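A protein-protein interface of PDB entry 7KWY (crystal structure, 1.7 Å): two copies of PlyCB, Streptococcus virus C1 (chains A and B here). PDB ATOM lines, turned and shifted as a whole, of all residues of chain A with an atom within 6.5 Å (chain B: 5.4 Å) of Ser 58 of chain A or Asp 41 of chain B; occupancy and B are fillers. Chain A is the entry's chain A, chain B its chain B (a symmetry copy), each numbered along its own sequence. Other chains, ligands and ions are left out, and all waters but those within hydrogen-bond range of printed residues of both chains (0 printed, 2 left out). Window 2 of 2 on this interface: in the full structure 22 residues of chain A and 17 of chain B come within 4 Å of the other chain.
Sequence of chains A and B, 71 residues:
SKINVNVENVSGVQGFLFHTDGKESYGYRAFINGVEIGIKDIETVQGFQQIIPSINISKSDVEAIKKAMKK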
ATOM      1  N   HIS A  19      13.903 -24.990 -17.317  1.00  0.00           N
ATOM      2  CA  HIS A  19      15.151 -24.635 -16.643  1.00  0.00           C
ATOM      3  C   HIS A  19      14.853 -24.611 -15.150  1.00  0.00           C
ATOM      4  O   HIS A  19      13.690 -24.604 -14.752  1.00  0.00           O
ATOM      5  CB  HIS A  19      15.669 -23.269 -17.107  1.00  0.00           C
ATOM      6  CG  HIS A  19      14.883 -22.111 -16.579  1.00  0.00           C
ATOM      7  ND1 HIS A  19      13.641 -21.780 -17.068  1.00  0.00           N
ATOM      8  CD2 HIS A  19      15.146 -21.224 -15.585  1.00  0.00           C
ATOM      9  CE1 HIS A  19      13.171 -20.732 -16.411  1.00  0.00           C
ATOM     10  NE2 HIS A  19      14.063 -20.367 -15.511  1.00  0.00           N
ATOM     11  N   THR A  20      15.915 -24.529 -14.322  1.00  0.00           N
ATOM     12  CA  THR A  20      15.699 -24.270 -12.896  1.00  0.00           C
ATOM     13  C   THR A  20      16.318 -22.947 -12.480  1.00  0.00           C
ATOM     14  O   THR A  20      17.370 -22.545 -12.988  1.00  0.00           O
ATOM     15  CB  THR A  20      16.276 -25.390 -12.001  1.00  0.00           C
ATOM     16  OG1 THR A  20      16.030 -25.082 -10.610  1.00  0.00           O
ATOM     17  CG2 THR A  20      17.813 -25.588 -12.198  1.00  0.00           C
ATOM     18  N   LYS A  23      19.458 -23.978  -6.963  1.00  0.00           N
ATOM     19  CA  LYS A  23      20.877 -24.259  -6.987  1.00  0.00           C
ATOM     20  C   LYS A  23      21.128 -25.339  -8.038  1.00  0.00           C
ATOM     21  O   LYS A  23      20.247 -26.155  -8.364  1.00  0.00           O
ATOM     22  CB  LYS A  23      21.378 -24.664  -5.589  1.00  0.00           C
ATOM     23  N   TYR A  26      21.014 -26.326 -14.797  1.00  0.00           N
ATOM     24  CA  TYR A  26      21.378 -27.205 -15.904  1.00  0.00           C
ATOM     25  C   TYR A  26      21.204 -26.492 -17.228  1.00  0.00           C
ATOM     26  O   TYR A  26      21.118 -27.138 -18.288  1.00  0.00           O
ATOM     27  CB  TYR A  26      20.577 -28.514 -15.893  1.00  0.00           C
ATOM     28  CG  TYR A  26      19.079 -28.325 -15.770  1.00  0.00           C
ATOM     29  CD1 TYR A  26      18.304 -28.050 -16.893  1.00  0.00           C
ATOM     30  CD2 TYR A  26      18.481 -28.393 -14.534  1.00  0.00           C
ATOM     31  CE1 TYR A  26      16.924 -27.878 -16.787  1.00  0.00           C
ATOM     32  CE2 TYR A  26      17.094 -28.223 -14.389  1.00  0.00           C
ATOM     33  CZ  TYR A  26      16.328 -27.947 -15.526  1.00  0.00           C
ATOM     34  OH  TYR A  26      14.955 -27.748 -15.406  1.00  0.00           O
ATOM     35  N   ASN A  56       9.458 -23.872 -15.251  1.00  0.00           N
ATOM     36  CA  ASN A  56      10.529 -24.203 -14.312  1.00  0.00           C
ATOM     37  C   ASN A  56      10.402 -25.642 -13.819  1.00  0.00           C
ATOM     38  O   ASN A  56       9.299 -26.080 -13.475  1.00  0.00           O
ATOM     39  CB  ASN A  56      10.454 -23.284 -13.092  1.00  0.00           C
ATOM     40  CG  ASN A  56      10.917 -21.870 -13.386  1.00  0.00           C
ATOM     41  OD1 ASN A  56      10.273 -21.143 -14.141  1.00  0.00           O
ATOM     42  ND2 ASN A  56      11.972 -21.435 -12.690  1.00  0.00           N
ATOM     43  N   ILE A  57      11.506 -26.373 -13.824  1.00  0.00           N
ATOM     44  CA  ILE A  57      11.558 -27.747 -13.311  1.00  0.00           C
ATOM     45  C   ILE A  57      12.817 -27.861 -12.474  1.00  0.00           C
ATOM     46  O   ILE A  57      13.919 -27.603 -12.979  1.00  0.00           O
ATOM     47  CB  ILE A  57      11.572 -28.794 -14.450  1.00  0.00           C
ATOM     48  CG1 ILE A  57      10.320 -28.644 -15.333  1.00  0.00           C
ATOM     49  CG2 ILE A  57      11.664 -30.191 -13.867  1.00  0.00           C
ATOM     50  CD1 ILE A  57      10.215 -29.740 -16.450  1.00  0.00           C
ATOM     51  N   SER A  58      12.679 -28.277 -11.218  1.00  0.00           N
ATOM     52  CA  SER A  58      13.880 -28.484 -10.395  1.00  0.00           C
ATOM     53  C   SER A  58      14.790 -29.534 -11.011  1.00  0.00           C
ATOM     54  O   SER A  58      14.328 -30.512 -11.608  1.00  0.00           O
ATOM     55  CB  SER A  58      13.452 -28.976  -9.013  1.00  0.00           C
ATOM     56  OG  SER A  58      14.540 -29.096  -8.152  1.00  0.00           O
ATOM     57  N   LYS A  59      16.101 -29.387 -10.786  1.00  0.00           N
ATOM     58  CA  LYS A  59      17.033 -30.421 -11.259  1.00  0.00           C
ATOM     59  C   LYS A  59      16.641 -31.818 -10.757  1.00  0.00           C
ATOM     60  O   LYS A  59      16.720 -32.800 -11.504  1.00  0.00           O
ATOM     61  CB  LYS A  59      18.457 -30.073 -10.815  1.00  0.00           C
ATOM     62  CG  LYS A  59      19.527 -31.056 -11.310  1.00  0.00           C
ATOM     63  CD  LYS A  59      20.924 -30.614 -10.895  1.00  0.00           C
ATOM     64  CE  LYS A  59      21.970 -31.656 -11.329  1.00  0.00           C
ATOM     65  NZ  LYS A  59      23.340 -31.348 -10.843  1.00  0.00           N
ATOM     66  N   SER A  60      16.151 -31.909  -9.514  1.00  0.00           N
ATOM     67  CA  SER A  60      15.822 -33.196  -8.895  1.00  0.00           C
ATOM     68  C   SER A  60      14.602 -33.855  -9.544  1.00  0.00           C
ATOM     69  O   SER A  60      14.389 -35.067  -9.369  1.00  0.00           O
ATOM     70  CB  SER A  60      15.546 -33.006  -7.402  1.00  0.00           C
ATOM     71  OG  SER A  60      14.401 -32.149  -7.221  1.00  0.00           O
ATOM     72  N   ASP A  61      13.808 -33.099 -10.286  1.00  0.00           N
ATOM     73  CA  ASP A  61      12.577 -33.629 -10.890  1.00  0.00           C
ATOM     74  C   ASP A  61      12.711 -33.962 -12.371  1.00  0.00           C
ATOM     75  O   ASP A  61      11.775 -34.531 -12.949  1.00  0.00           O
ATOM     76  CB  ASP A  61      11.436 -32.614 -10.716  1.00  0.00           C
ATOM     77  CG  ASP A  61      10.840 -32.665  -9.311  1.00  0.00           C
ATOM     78  OD1 ASP A  61      10.640 -33.797  -8.784  1.00  0.00           O
ATOM     79  OD2 ASP A  61      10.580 -31.593  -8.711  1.00  0.00           O
ATOM     80  N   VAL A  62      13.820 -33.593 -13.003  1.00  0.00           N
ATOM     81  CA  VAL A  62      13.977 -33.797 -14.434  1.00  0.00           C
ATOM     82  C   VAL A  62      13.872 -35.275 -14.805  1.00  0.00           C
ATOM     83  O   VAL A  62      13.240 -35.620 -15.812  1.00  0.00           O
ATOM     84  CB  VAL A  62      15.321 -33.208 -14.893  1.00  0.00           C
ATOM     85  CG1 VAL A  62      15.583 -33.628 -16.331  1.00  0.00           C
ATOM     86  CG2 VAL A  62      15.234 -31.664 -14.801  1.00  0.00           C
ATOM     87  N   GLU A  63      14.460 -36.172 -14.005  1.00  0.00           N
ATOM     88  CA  GLU A  63      14.438 -37.580 -14.417  1.00  0.00           C
ATOM     89  C   GLU A  63      13.012 -38.117 -14.468  1.00  0.00           C
ATOM     90  O   GLU A  63      12.631 -38.813 -15.414  1.00  0.00           O
ATOM     91  CB  GLU A  63      15.292 -38.443 -13.477  1.00  0.00           C
ATOM     92  CG  GLU A  63      16.799 -38.231 -13.657  1.00  0.00           C
ATOM     93  CD  GLU A  63      17.298 -38.552 -15.069  1.00  0.00           C
ATOM     94  OE1 GLU A  63      18.117 -37.764 -15.597  1.00  0.00           O
ATOM     95  OE2 GLU A  63      16.881 -39.587 -15.645  1.00  0.00           O
ATOM     96  N   ILE B  39       6.450 -35.608  -7.451  1.00  0.00           N
ATOM     97  CA  ILE B  39       7.134 -34.343  -7.698  1.00  0.00           C
ATOM     98  C   ILE B  39       7.871 -33.985  -6.416  1.00  0.00           C
ATOM     99  O   ILE B  39       7.266 -33.935  -5.340  1.00  0.00           O
ATOM    100  CB  ILE B  39       6.154 -33.224  -8.098  1.00  0.00           C
ATOM    101  CG1 ILE B  39       5.242 -33.608  -9.252  1.00  0.00           C
ATOM    102  CG2 ILE B  39       6.916 -31.896  -8.361  1.00  0.00           C
ATOM    103  CD1 ILE B  39       5.936 -33.858 -10.550  1.00  0.00           C
ATOM    104  N   LYS B  40       9.168 -33.735  -6.509  1.00  0.00           N
ATOM    105  CA  LYS B  40       9.936 -33.501  -5.282  1.00  0.00           C
ATOM    106  C   LYS B  40       9.988 -32.043  -4.836  1.00  0.00           C
ATOM    107  O   LYS B  40      10.075 -31.780  -3.628  1.00  0.00           O
ATOM    108  CB  LYS B  40      11.374 -34.001  -5.472  1.00  0.00           C
ATOM    109  CG  LYS B  40      11.465 -35.506  -5.740  1.00  0.00           C
ATOM    110  CD  LYS B  40      12.902 -35.891  -6.065  1.00  0.00           C
ATOM    111  CE  LYS B  40      13.003 -37.238  -6.774  1.00  0.00           C
ATOM    112  NZ  LYS B  40      12.366 -38.347  -6.019  1.00  0.00           N
ATOM    113  N   ASP B  41       9.948 -31.088  -5.753  1.00  0.00           N
ATOM    114  CA  ASP B  41      10.307 -29.697  -5.448  1.00  0.00           C
ATOM    115  C   ASP B  41       9.158 -28.767  -5.799  1.00  0.00           C
ATOM    116  O   ASP B  41       8.526 -28.935  -6.841  1.00  0.00           O
ATOM    117  CB  ASP B  41      11.552 -29.297  -6.250  1.00  0.00           C
ATOM    118  CG  ASP B  41      12.266 -28.035  -5.712  1.00  0.00           C
ATOM    119  OD1 ASP B  41      11.701 -26.899  -5.679  1.00  0.00           O
ATOM    120  OD2 ASP B  41      13.451 -28.193  -5.351  1.00  0.00           O
ATOM    121  N   ILE B  42       8.898 -27.754  -4.964  1.00  0.00           N
ATOM    122  CA  ILE B  42       7.751 -26.876  -5.257  1.00  0.00           C
ATOM    123  C   ILE B  42       8.004 -26.067  -6.509  1.00  0.00           C
ATOM    124  O   ILE B  42       7.051 -25.589  -7.134  1.00  0.00           O
ATOM    125  CB  ILE B  42       7.462 -25.944  -4.054  1.00  0.00           C
ATOM    126  CG1 ILE B  42       6.104 -25.235  -4.182  1.00  0.00           C
ATOM    127  CG2 ILE B  42       8.516 -24.902  -3.880  1.00  0.00           C
ATOM    128  CD1 ILE B  42       4.853 -26.112  -4.107  1.00  0.00           C
ATOM    129  N   GLU B  43       9.271 -25.878  -6.876  1.00  0.00           N
ATOM    130  CA  GLU B  43       9.514 -25.128  -8.125  1.00  0.00           C
ATOM    131  C   GLU B  43       8.855 -25.833  -9.296  1.00  0.00           C
ATOM    132  O   GLU B  43       8.256 -25.193 -10.185  1.00  0.00           O
ATOM    133  CB  GLU B  43      11.020 -24.978  -8.367  1.00  0.00           C
ATOM    134  CG  GLU B  43      11.315 -24.251  -9.731  1.00  0.00           C
ATOM    135  CD  GLU B  43      12.798 -24.191 -10.080  1.00  0.00           C
ATOM    136  OE1 GLU B  43      13.589 -25.073  -9.656  1.00  0.00           O
ATOM    137  OE2 GLU B  43      13.181 -23.232 -10.797  1.00  0.00           O
ATOM    138  N   THR B  44       8.992 -27.163  -9.314  1.00  0.00           N
ATOM    139  CA  THR B  44       8.414 -27.991 -10.375  1.00  0.00           C
ATOM    140  C   THR B  44       6.900 -27.965 -10.311  1.00  0.00           C
ATOM    141  O   THR B  44       6.240 -27.925 -11.348  1.00  0.00           O
ATOM    142  CB  THR B  44       8.911 -29.430 -10.224  1.00  0.00           C
ATOM    143  OG1 THR B  44      10.353 -29.456 -10.147  1.00  0.00           O
ATOM    144  CG2 THR B  44       8.444 -30.301 -11.437  1.00  0.00           C
ATOM    145  N   VAL B  45       6.324 -28.010  -9.114  1.00  0.00           N
ATOM    146  CA  VAL B  45       4.868 -27.861  -8.999  1.00  0.00           C
ATOM    147  C   VAL B  45       4.397 -26.561  -9.639  1.00  0.00           C
ATOM    148  O   VAL B  45       3.441 -26.543 -10.412  1.00  0.00           O
ATOM    149  CB  VAL B  45       4.442 -27.905  -7.528  1.00  0.00           C
ATOM    150  CG1 VAL B  45       2.904 -27.633  -7.437  1.00  0.00           C
ATOM    151  CG2 VAL B  45       4.800 -29.269  -6.994  1.00  0.00           C
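The side-chain hydroxyl of Thr 20 of chain A sits at hydrogen-bond distance from the side-chain carboxylate of Glu 43 of chain B, 2.6 Å away. The side-chain amide nitrogen of Asn 56 of chain A is in hydrogen-bond range of the side-chain carboxylate of Glu 43 of chain B (2.9 Å). The side-chain hydroxyl (OG) of Ser 58 of chain A sits at hydrogen-bond distance from the side-chain carboxylate (OD2) of Asp 41 of chain B, at 3.1 Å. The backbone NH of Ser 58 of chain A sits at hydrogen-bond distance from the side-chain hydroxyl of Thr 44 of chain B (2.8 Å). OD1 of Asp 61 of chain A lies within hydrogen-bond range of N of Lys 40 of chain B, at 2.7 Å. OD2 of Asp 61 of chain A is in hydrogen-bond range of N of Asp 41 of chain B. The side-chain carboxylate (OD2) of Asp 61 of chain A is in hydrogen-bond range of the side-chain hydroxyl (OG1) of Thr 44 of chain B (2.6 Å).
The backbone NH (N) of Ile 57 of chain A is in hydrogen-bond range of the backbone carbonyl oxygen (O) of His 19 of chain A, 3.0 Å away. OH of Tyr 26 of chain A lies within hydrogen-bond range of O of Ile 57 of chain A. The side-chain hydroxyl (OG) of Ser 58 of chain A sits at hydrogen-bond distance from the side-chain hydroxyl (OG) of Ser 60 of chain A (3.2 Å). The backbone NH (N) of Glu 43 of chain B sits at hydrogen-bond distance from the side-chain carboxylate (OD1) of Asp 41 of chain B (2.9 Å).
Among the printed residues, pairs that only touch across the chains: Asn 56 of chain A with Thr 44 of chain B, Ile 57 of chain A with Thr 44 of chain B, Ser 58 of chain A with Glu 43 of chain B, Ser 60 of chain A with Lys 40 of chain B and Asp 61 of chain A with Ile 39 of chain B.
Of chain A, only Ser 58 (3.1 Å) and Asp 61 (3.1 Å) come within 4 Å of Asp 41 of chain B. Printed residues of chain A within 4 Å of Ile 39 of chain B: Asp 61 (3.6 Å). Of the printed residues of chain B, Thr 20 of chain A touches Glu 43 (2.6 Å). Lys 23 of chain A touches none of the printed residues of chain B. Tyr 26 of chain A touches none of the printed residues of chain B. The nearest printed residue of chain B that does not touch Ser 58 of chain A is Ile 42 of chain B (6.2 Å). The nearest residue of chain A that does not touch Asp 41 of chain B is Ser 60 of chain A (4.1 Å). The nearest printed residue of chain A that does not touch Glu 43 of chain B is Ile 57 of chain A (4.04 Å).
Printed residues of chain A that touch a printed residue of chain B: Thr 20, Asn 56, Ile 57, Ser 58, Ser 60 and Asp 61. Along chain A the printed residues that touch a printed residue of chain B span positions 20 to 61. Hydrophobic or aromatic side chains of chain B that line the printed part of chain A: Ile 39. Among the printed residues, no Asp or Glu carboxylate lies within 4 Å of a Lys or Arg side-chain nitrogen of the other chain.
No position is printed for both chains. Of the 12 pairs that touch across the chains among the printed residues, none has its exchanged pair printed and touching as well.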
